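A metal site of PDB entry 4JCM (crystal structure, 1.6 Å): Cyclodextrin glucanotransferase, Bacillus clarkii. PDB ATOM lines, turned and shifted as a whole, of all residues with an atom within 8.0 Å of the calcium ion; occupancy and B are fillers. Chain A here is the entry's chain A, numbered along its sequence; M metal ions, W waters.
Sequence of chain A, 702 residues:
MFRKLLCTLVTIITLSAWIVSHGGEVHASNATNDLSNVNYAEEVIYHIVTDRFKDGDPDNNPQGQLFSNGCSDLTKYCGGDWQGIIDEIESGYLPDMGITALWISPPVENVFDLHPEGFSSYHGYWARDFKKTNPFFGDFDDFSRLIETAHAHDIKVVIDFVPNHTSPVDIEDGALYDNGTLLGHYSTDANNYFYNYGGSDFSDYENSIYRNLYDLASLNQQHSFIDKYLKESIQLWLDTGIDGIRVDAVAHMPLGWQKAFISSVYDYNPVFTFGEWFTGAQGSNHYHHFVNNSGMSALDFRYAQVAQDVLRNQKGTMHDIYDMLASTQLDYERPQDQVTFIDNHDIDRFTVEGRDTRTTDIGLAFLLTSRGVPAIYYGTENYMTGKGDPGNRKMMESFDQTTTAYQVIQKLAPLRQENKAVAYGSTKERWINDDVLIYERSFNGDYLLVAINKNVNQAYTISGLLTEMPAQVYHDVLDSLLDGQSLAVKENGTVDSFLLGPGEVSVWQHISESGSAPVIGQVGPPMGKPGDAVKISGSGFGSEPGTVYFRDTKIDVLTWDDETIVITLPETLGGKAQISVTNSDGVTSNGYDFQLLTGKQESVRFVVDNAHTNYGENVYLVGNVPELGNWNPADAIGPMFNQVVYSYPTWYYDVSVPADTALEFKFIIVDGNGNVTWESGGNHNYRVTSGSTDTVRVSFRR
The backbone carbonyl oxygen of Pro 58 lies close to the side-chain amide nitrogen of Asn 61 (3.4 Å). N of Gly 56 sits at hydrogen-bond distance from OD1 of Asp 81 (2.9 Å). N of Asp 81 lies within hydrogen-bond range of O of Lys 54, 3.0 Å away. The side-chain carboxylate of Asp 81 lies close to the backbone NH of Gln 83, 3.3 Å away. OD1 of Asp 81 lies within hydrogen-bond range of N of Gly 84 (2.9 Å). The backbone carbonyl oxygen (O) of Phe 136 sits close to the side-chain amide oxygen (OD1) of Asn 60, at 3.1 Å. The side-chain carboxylate (OD1) of Asp 51 lies within hydrogen-bond range of the backbone NH (N) of Gly 79, 3.0 Å away. The side-chain carboxylate of Asp 57 sits close to the backbone NH of Asp 59 (3.1 Å).
Of the 25 residues printed, 6 come within 4 Å of the calcium ion.
The calcium ion is bound by OD1 of Asn 61 (2.4 Å). The calcium ion is bound by the side-chain carboxylate (OD2) of Asp 81, at 2.4 Å. OD1 of Asn 60 binds the calcium ion (2.5 Å). O of Gly 79 is bound to the calcium ion (2.5 Å). OD1 of Asp 55 is bound to the calcium ion, 2.6 Å away. Water W1 is bound to the calcium ion (2.6 Å). O of Asp 57 is bound to the calcium ion (2.7 Å). The calcium ion has seven donor atoms within binding distance.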
ATOM      1  N   THR A  50     -12.962 -24.884  15.430  1.00  0.00           N
ATOM      2  CA  THR A  50     -14.052 -24.857  14.456  1.00  0.00           C
ATOM      3  C   THR A  50     -13.595 -24.811  13.000  1.00  0.00           C
ATOM      4  O   THR A  50     -14.075 -25.580  12.160  1.00  0.00           O
ATOM      5  CB  THR A  50     -15.025 -23.718  14.760  1.00  0.00           C
ATOM      6  OG1 THR A  50     -15.525 -23.893  16.101  1.00  0.00           O
ATOM      7  CG2 THR A  50     -16.201 -23.735  13.782  1.00  0.00           C
ATOM      8  N   ASP A  51     -12.647 -23.930  12.712  1.00  0.00           N
ATOM      9  CA  ASP A  51     -12.174 -23.740  11.342  1.00  0.00           C
ATOM     10  C   ASP A  51     -11.486 -24.977  10.773  1.00  0.00           C
ATOM     11  O   ASP A  51     -11.367 -25.129   9.551  1.00  0.00           O
ATOM     12  CB  ASP A  51     -11.214 -22.563  11.279  1.00  0.00           C
ATOM     13  CG  ASP A  51     -10.753 -22.294   9.866  1.00  0.00           C
ATOM     14  OD1 ASP A  51     -11.593 -21.880   9.044  1.00  0.00           O
ATOM     15  OD2 ASP A  51      -9.548 -22.479   9.588  1.00  0.00           O
ATOM     16  N   LYS A  54     -14.585 -29.415  10.094  1.00  0.00           N
ATOM     17  CA  LYS A  54     -15.244 -29.758   8.831  1.00  0.00           C
ATOM     18  C   LYS A  54     -15.950 -28.576   8.186  1.00  0.00           C
ATOM     19  O   LYS A  54     -16.744 -27.885   8.822  1.00  0.00           O
ATOM     20  CB  LYS A  54     -16.235 -30.915   8.994  1.00  0.00           C
ATOM     21  CG  LYS A  54     -16.874 -31.317   7.663  1.00  0.00           C
ATOM     22  CD  LYS A  54     -17.887 -32.442   7.810  1.00  0.00           C
ATOM     23  CE  LYS A  54     -18.581 -32.740   6.489  1.00  0.00           C
ATOM     24  NZ  LYS A  54     -17.604 -33.093   5.422  1.00  0.00           N
ATOM     25  N   ASP A  55     -15.642 -28.365   6.917  1.00  0.00           N
ATOM     26  CA  ASP A  55     -16.308 -27.340   6.120  1.00  0.00           C
ATOM     27  C   ASP A  55     -17.642 -27.900   5.635  1.00  0.00           C
ATOM     28  O   ASP A  55     -17.717 -28.541   4.577  1.00  0.00           O
ATOM     29  CB  ASP A  55     -15.414 -26.943   4.933  1.00  0.00           C
ATOM     30  CG  ASP A  55     -16.015 -25.851   4.068  1.00  0.00           C
ATOM     31  OD1 ASP A  55     -17.101 -25.348   4.421  1.00  0.00           O
ATOM     32  OD2 ASP A  55     -15.410 -25.502   3.031  1.00  0.00           O
ATOM     33  N   GLY A  56     -18.693 -27.677   6.420  1.00  0.00           N
ATOM     34  CA  GLY A  56     -20.011 -28.176   6.082  1.00  0.00           C
ATOM     35  C   GLY A  56     -20.757 -27.263   5.131  1.00  0.00           C
ATOM     36  O   GLY A  56     -21.721 -27.668   4.483  1.00  0.00           O
ATOM     37  N   ASP A  57     -20.305 -26.016   5.047  1.00  0.00           N
ATOM     38  CA  ASP A  57     -20.953 -25.037   4.180  1.00  0.00           C
ATOM     39  C   ASP A  57     -19.907 -24.192   3.459  1.00  0.00           C
ATOM     40  O   ASP A  57     -19.537 -23.127   3.922  1.00  0.00           O
ATOM     41  CB  ASP A  57     -21.881 -24.155   5.010  1.00  0.00           C
ATOM     42  CG  ASP A  57     -22.621 -23.131   4.169  1.00  0.00           C
ATOM     43  OD1 ASP A  57     -22.510 -23.179   2.923  1.00  0.00           O
ATOM     44  OD2 ASP A  57     -23.324 -22.280   4.758  1.00  0.00           O
ATOM     45  N   PRO A  58     -19.439 -24.675   2.296  1.00  0.00           N
ATOM     46  CA  PRO A  58     -18.416 -23.930   1.547  1.00  0.00           C
ATOM     47  C   PRO A  58     -18.842 -22.501   1.205  1.00  0.00           C
ATOM     48  O   PRO A  58     -17.989 -21.638   0.994  1.00  0.00           O
ATOM     49  CB  PRO A  58     -18.271 -24.751   0.262  1.00  0.00           C
ATOM     50  CG  PRO A  58     -18.653 -26.135   0.664  1.00  0.00           C
ATOM     51  CD  PRO A  58     -19.758 -25.971   1.664  1.00  0.00           C
ATOM     52  N   ASP A  59     -20.149 -22.254   1.168  1.00  0.00           N
ATOM     53  CA  ASP A  59     -20.666 -20.940   0.792  1.00  0.00           C
ATOM     54  C   ASP A  59     -20.344 -19.829   1.800  1.00  0.00           C
ATOM     55  O   ASP A  59     -20.299 -18.654   1.423  1.00  0.00           O
ATOM     56  CB  ASP A  59     -22.165 -21.000   0.517  1.00  0.00           C
ATOM     57  CG  ASP A  59     -22.501 -21.818  -0.723  1.00  0.00           C
ATOM     58  OD1 ASP A  59     -23.595 -22.415  -0.774  1.00  0.00           O
ATOM     59  OD2 ASP A  59     -21.661 -21.868  -1.649  1.00  0.00           O
ATOM     60  N   ASN A  60     -20.128 -20.185   3.060  1.00  0.00           N
ATOM     61  CA  ASN A  60     -19.748 -19.160   4.034  1.00  0.00           C
ATOM     62  C   ASN A  60     -18.222 -19.011   4.164  1.00  0.00           C
ATOM     63  O   ASN A  60     -17.737 -18.258   4.992  1.00  0.00           O
ATOM     64  CB  ASN A  60     -20.430 -19.386   5.395  1.00  0.00           C
ATOM     65  CG  ASN A  60     -19.976 -20.659   6.072  1.00  0.00           C
ATOM     66  OD1 ASN A  60     -18.873 -21.136   5.828  1.00  0.00           O
ATOM     67  ND2 ASN A  60     -20.819 -21.210   6.934  1.00  0.00           N
ATOM     68  N   ASN A  61     -17.487 -19.714   3.313  1.00  0.00           N
ATOM     69  CA  ASN A  61     -16.026 -19.592   3.317  1.00  0.00           C
ATOM     70  C   ASN A  61     -15.594 -18.168   3.000  1.00  0.00           C
ATOM     71  O   ASN A  61     -16.194 -17.511   2.158  1.00  0.00           O
ATOM     72  CB  ASN A  61     -15.411 -20.516   2.274  1.00  0.00           C
ATOM     73  CG  ASN A  61     -15.412 -21.964   2.713  1.00  0.00           C
ATOM     74  OD1 ASN A  61     -15.840 -22.278   3.818  1.00  0.00           O
ATOM     75  ND2 ASN A  61     -14.929 -22.857   1.857  1.00  0.00           N
ATOM     76  N   PRO A  62     -14.531 -17.686   3.666  1.00  0.00           N
ATOM     77  CA  PRO A  62     -13.956 -16.410   3.239  1.00  0.00           C
ATOM     78  C   PRO A  62     -13.472 -16.524   1.803  1.00  0.00           C
ATOM     79  O   PRO A  62     -13.210 -17.629   1.332  1.00  0.00           O
ATOM     80  CB  PRO A  62     -12.749 -16.226   4.158  1.00  0.00           C
ATOM     81  CG  PRO A  62     -12.963 -17.145   5.303  1.00  0.00           C
ATOM     82  CD  PRO A  62     -13.784 -18.292   4.786  1.00  0.00           C
ATOM     83  N   PHE A  67      -8.542 -16.783   3.027  1.00  0.00           N
ATOM     84  CA  PHE A  67      -8.827 -18.207   2.842  1.00  0.00           C
ATOM     85  C   PHE A  67      -7.644 -18.973   2.261  1.00  0.00           C
ATOM     86  O   PHE A  67      -6.957 -18.495   1.354  1.00  0.00           O
ATOM     87  CB  PHE A  67     -10.048 -18.376   1.933  1.00  0.00           C
ATOM     88  CG  PHE A  67     -10.508 -19.794   1.798  1.00  0.00           C
ATOM     89  CD1 PHE A  67     -11.111 -20.441   2.861  1.00  0.00           C
ATOM     90  CD2 PHE A  67     -10.357 -20.478   0.604  1.00  0.00           C
ATOM     91  CE1 PHE A  67     -11.544 -21.761   2.741  1.00  0.00           C
ATOM     92  CE2 PHE A  67     -10.779 -21.785   0.469  1.00  0.00           C
ATOM     93  CZ  PHE A  67     -11.382 -22.431   1.533  1.00  0.00           C
ATOM     94  N   TYR A  77      -7.996 -18.940   7.255  1.00  0.00           N
ATOM     95  CA  TYR A  77      -9.223 -19.711   7.374  1.00  0.00           C
ATOM     96  C   TYR A  77      -9.183 -20.857   6.374  1.00  0.00           C
ATOM     97  O   TYR A  77      -8.871 -20.639   5.185  1.00  0.00           O
ATOM     98  CB  TYR A  77     -10.435 -18.849   7.069  1.00  0.00           C
ATOM     99  CG  TYR A  77     -10.927 -17.971   8.202  1.00  0.00           C
ATOM    100  CD1 TYR A  77     -10.318 -16.751   8.490  1.00  0.00           C
ATOM    101  CD2 TYR A  77     -12.032 -18.346   8.970  1.00  0.00           C
ATOM    102  CE1 TYR A  77     -10.779 -15.945   9.507  1.00  0.00           C
ATOM    103  CE2 TYR A  77     -12.503 -17.542   9.986  1.00  0.00           C
ATOM    104  CZ  TYR A  77     -11.877 -16.344  10.259  1.00  0.00           C
ATOM    105  OH  TYR A  77     -12.346 -15.548  11.269  1.00  0.00           O
ATOM    106  N   CYS A  78      -9.527 -22.055   6.831  1.00  0.00           N
ATOM    107  CA  CYS A  78      -9.592 -23.226   5.965  1.00  0.00           C
ATOM    108  C   CYS A  78     -11.020 -23.663   5.676  1.00  0.00           C
ATOM    109  O   CYS A  78     -11.248 -24.526   4.814  1.00  0.00           O
ATOM    110  CB  CYS A  78      -8.794 -24.361   6.578  1.00  0.00           C
ATOM    111  SG  CYS A  78      -7.054 -23.921   6.735  1.00  0.00           S
ATOM    112  N   GLY A  79     -11.977 -23.092   6.382  1.00  0.00           N
ATOM    113  CA  GLY A  79     -13.372 -23.298   6.032  1.00  0.00           C
ATOM    114  C   GLY A  79     -14.251 -24.057   7.010  1.00  0.00           C
ATOM    115  O   GLY A  79     -15.457 -24.120   6.811  1.00  0.00           O
ATOM    116  N   GLY A  80     -13.658 -24.634   8.051  1.00  0.00           N
ATOM    117  CA  GLY A  80     -14.448 -25.369   9.029  1.00  0.00           C
ATOM    118  C   GLY A  80     -15.523 -24.503   9.670  1.00  0.00           C
ATOM    119  O   GLY A  80     -15.293 -23.337   9.995  1.00  0.00           O
ATOM    120  N   ASP A  81     -16.714 -25.075   9.843  1.00  0.00           N
ATOM    121  CA  ASP A  81     -17.848 -24.266  10.297  1.00  0.00           C
ATOM    122  C   ASP A  81     -18.842 -25.063  11.147  1.00  0.00           C
ATOM    123  O   ASP A  81     -18.627 -26.246  11.405  1.00  0.00           O
ATOM    124  CB  ASP A  81     -18.536 -23.601   9.101  1.00  0.00           C
ATOM    125  CG  ASP A  81     -18.973 -24.616   8.041  1.00  0.00           C
ATOM    126  OD1 ASP A  81     -19.355 -25.736   8.428  1.00  0.00           O
ATOM    127  OD2 ASP A  81     -18.936 -24.306   6.833  1.00  0.00           O
ATOM    128  N   TRP A  82     -19.911 -24.410  11.578  1.00  0.00           N
ATOM    129  CA  TRP A  82     -20.879 -25.062  12.464  1.00  0.00           C
ATOM    130  C   TRP A  82     -21.678 -26.148  11.732  1.00  0.00           C
ATOM    131  O   TRP A  82     -22.003 -27.189  12.310  1.00  0.00           O
ATOM    132  CB  TRP A  82     -21.804 -24.034  13.128  1.00  0.00           C
ATOM    133  CG  TRP A  82     -21.052 -23.091  14.038  1.00  0.00           C
ATOM    134  CD1 TRP A  82     -19.910 -23.364  14.743  1.00  0.00           C
ATOM    135  CD2 TRP A  82     -21.359 -21.714  14.295  1.00  0.00           C
ATOM    136  NE1 TRP A  82     -19.509 -22.251  15.446  1.00  0.00           N
ATOM    137  CE2 TRP A  82     -20.370 -21.226  15.185  1.00  0.00           C
ATOM    138  CE3 TRP A  82     -22.373 -20.852  13.871  1.00  0.00           C
ATOM    139  CZ2 TRP A  82     -20.382 -19.915  15.658  1.00  0.00           C
ATOM    140  CZ3 TRP A  82     -22.376 -19.540  14.346  1.00  0.00           C
ATOM    141  CH2 TRP A  82     -21.379 -19.089  15.221  1.00  0.00           C
ATOM    142  N   GLN A  83     -21.977 -25.923  10.465  1.00  0.00           N
ATOM    143  CA  GLN A  83     -22.662 -26.941   9.682  1.00  0.00           C
ATOM    144  C   GLN A  83     -21.832 -28.233   9.639  1.00  0.00           C
ATOM    145  O   GLN A  83     -22.385 -29.325   9.666  1.00  0.00           O
ATOM    146  CB  GLN A  83     -22.987 -26.462   8.266  1.00  0.00           C
ATOM    147  CG  GLN A  83     -23.731 -27.494   7.429  1.00  0.00           C
ATOM    148  CD  GLN A  83     -25.094 -27.836   8.023  1.00  0.00           C
ATOM    149  OE1 GLN A  83     -25.884 -26.955   8.349  1.00  0.00           O
ATOM    150  NE2 GLN A  83     -25.367 -29.133   8.173  1.00  0.00           N
ATOM    151  N   GLY A  84     -20.517 -28.078   9.578  1.00  0.00           N
ATOM    152  CA  GLY A  84     -19.620 -29.228   9.573  1.00  0.00           C
ATOM    153  C   GLY A  84     -19.722 -30.034  10.865  1.00  0.00           C
ATOM    154  O   GLY A  84     -19.725 -31.260  10.843  1.00  0.00           O
ATOM    155  N   PRO A 135     -19.401 -14.795  10.847  1.00  0.00           N
ATOM    156  CA  PRO A 135     -20.220 -15.296   9.724  1.00  0.00           C
ATOM    157  C   PRO A 135     -19.529 -16.402   8.941  1.00  0.00           C
ATOM    158  O   PRO A 135     -20.182 -17.081   8.140  1.00  0.00           O
ATOM    159  CB  PRO A 135     -20.418 -14.057   8.857  1.00  0.00           C
ATOM    160  CG  PRO A 135     -19.229 -13.204   9.148  1.00  0.00           C
ATOM    161  CD  PRO A 135     -18.912 -13.434  10.601  1.00  0.00           C
ATOM    162  N   PHE A 136     -18.233 -16.599   9.166  1.00  0.00           N
ATOM    163  CA  PHE A 136     -17.537 -17.692   8.506  1.00  0.00           C
ATOM    164  C   PHE A 136     -17.867 -19.039   9.154  1.00  0.00           C
ATOM    165  O   PHE A 136     -17.764 -20.081   8.502  1.00  0.00           O
ATOM    166  CB  PHE A 136     -16.028 -17.452   8.503  1.00  0.00           C
ATOM    167  CG  PHE A 136     -15.626 -16.150   7.840  1.00  0.00           C
ATOM    168  CD1 PHE A 136     -16.116 -15.821   6.585  1.00  0.00           C
ATOM    169  CD2 PHE A 136     -14.772 -15.269   8.473  1.00  0.00           C
ATOM    170  CE1 PHE A 136     -15.762 -14.631   5.971  1.00  0.00           C
ATOM    171  CE2 PHE A 136     -14.410 -14.071   7.867  1.00  0.00           C
ATOM    172  CZ  PHE A 136     -14.896 -13.763   6.608  1.00  0.00           C
ATOM    173  N   PHE A 137     -18.275 -19.017  10.414  1.00  0.00           N
ATOM    174  CA  PHE A 137     -18.734 -20.227  11.104  1.00  0.00           C
ATOM    175  C   PHE A 137     -20.232 -20.446  10.872  1.00  0.00           C
ATOM    176  O   PHE A 137     -20.711 -21.580  10.863  1.00  0.00           O
ATOM    177  CB  PHE A 137     -18.445 -20.156  12.604  1.00  0.00           C
ATOM    178  CG  PHE A 137     -16.979 -20.042  12.967  1.00  0.00           C
ATOM    179  CD1 PHE A 137     -15.994 -20.343  12.040  1.00  0.00           C
ATOM    180  CD2 PHE A 137     -16.599 -19.611  14.234  1.00  0.00           C
ATOM    181  CE1 PHE A 137     -14.647 -20.230  12.379  1.00  0.00           C
ATOM    182  CE2 PHE A 137     -15.264 -19.491  14.576  1.00  0.00           C
ATOM    183  CZ  PHE A 137     -14.277 -19.800  13.643  1.00  0.00           C
ATOM    184  N   GLY A 138     -20.965 -19.351  10.701  1.00  0.00           N
ATOM    185  CA  GLY A 138     -22.399 -19.401  10.452  1.00  0.00           C
ATOM    186  C   GLY A 138     -23.131 -18.179  10.992  1.00  0.00           C
ATOM    187  O   GLY A 138     -22.515 -17.292  11.582  1.00  0.00           O
ATOM    188  N   MET A 395      -6.159 -29.373   9.462  1.00  0.00           N
ATOM    189  CA  MET A 395      -7.509 -29.775   9.119  1.00  0.00           C
ATOM    190  C   MET A 395      -7.717 -31.243   9.473  1.00  0.00           C
ATOM    191  O   MET A 395      -6.881 -32.089   9.152  1.00  0.00           O
ATOM    192  CB  MET A 395      -7.750 -29.575   7.613  1.00  0.00           C
ATOM    193  CG  MET A 395      -9.218 -29.491   7.237  1.00  0.00           C
ATOM    194  SD  MET A 395      -9.893 -27.861   7.638  1.00  0.00           S
ATOM    195  CE  MET A 395     -11.655 -28.181   7.570  1.00  0.00           C
HETATM  196 CA    CA M   1     -17.349 -23.029   5.509  1.00  0.00          CA
HETATM  197  O   HOH W   1     -16.026 -21.037   6.649  1.00  0.00           O
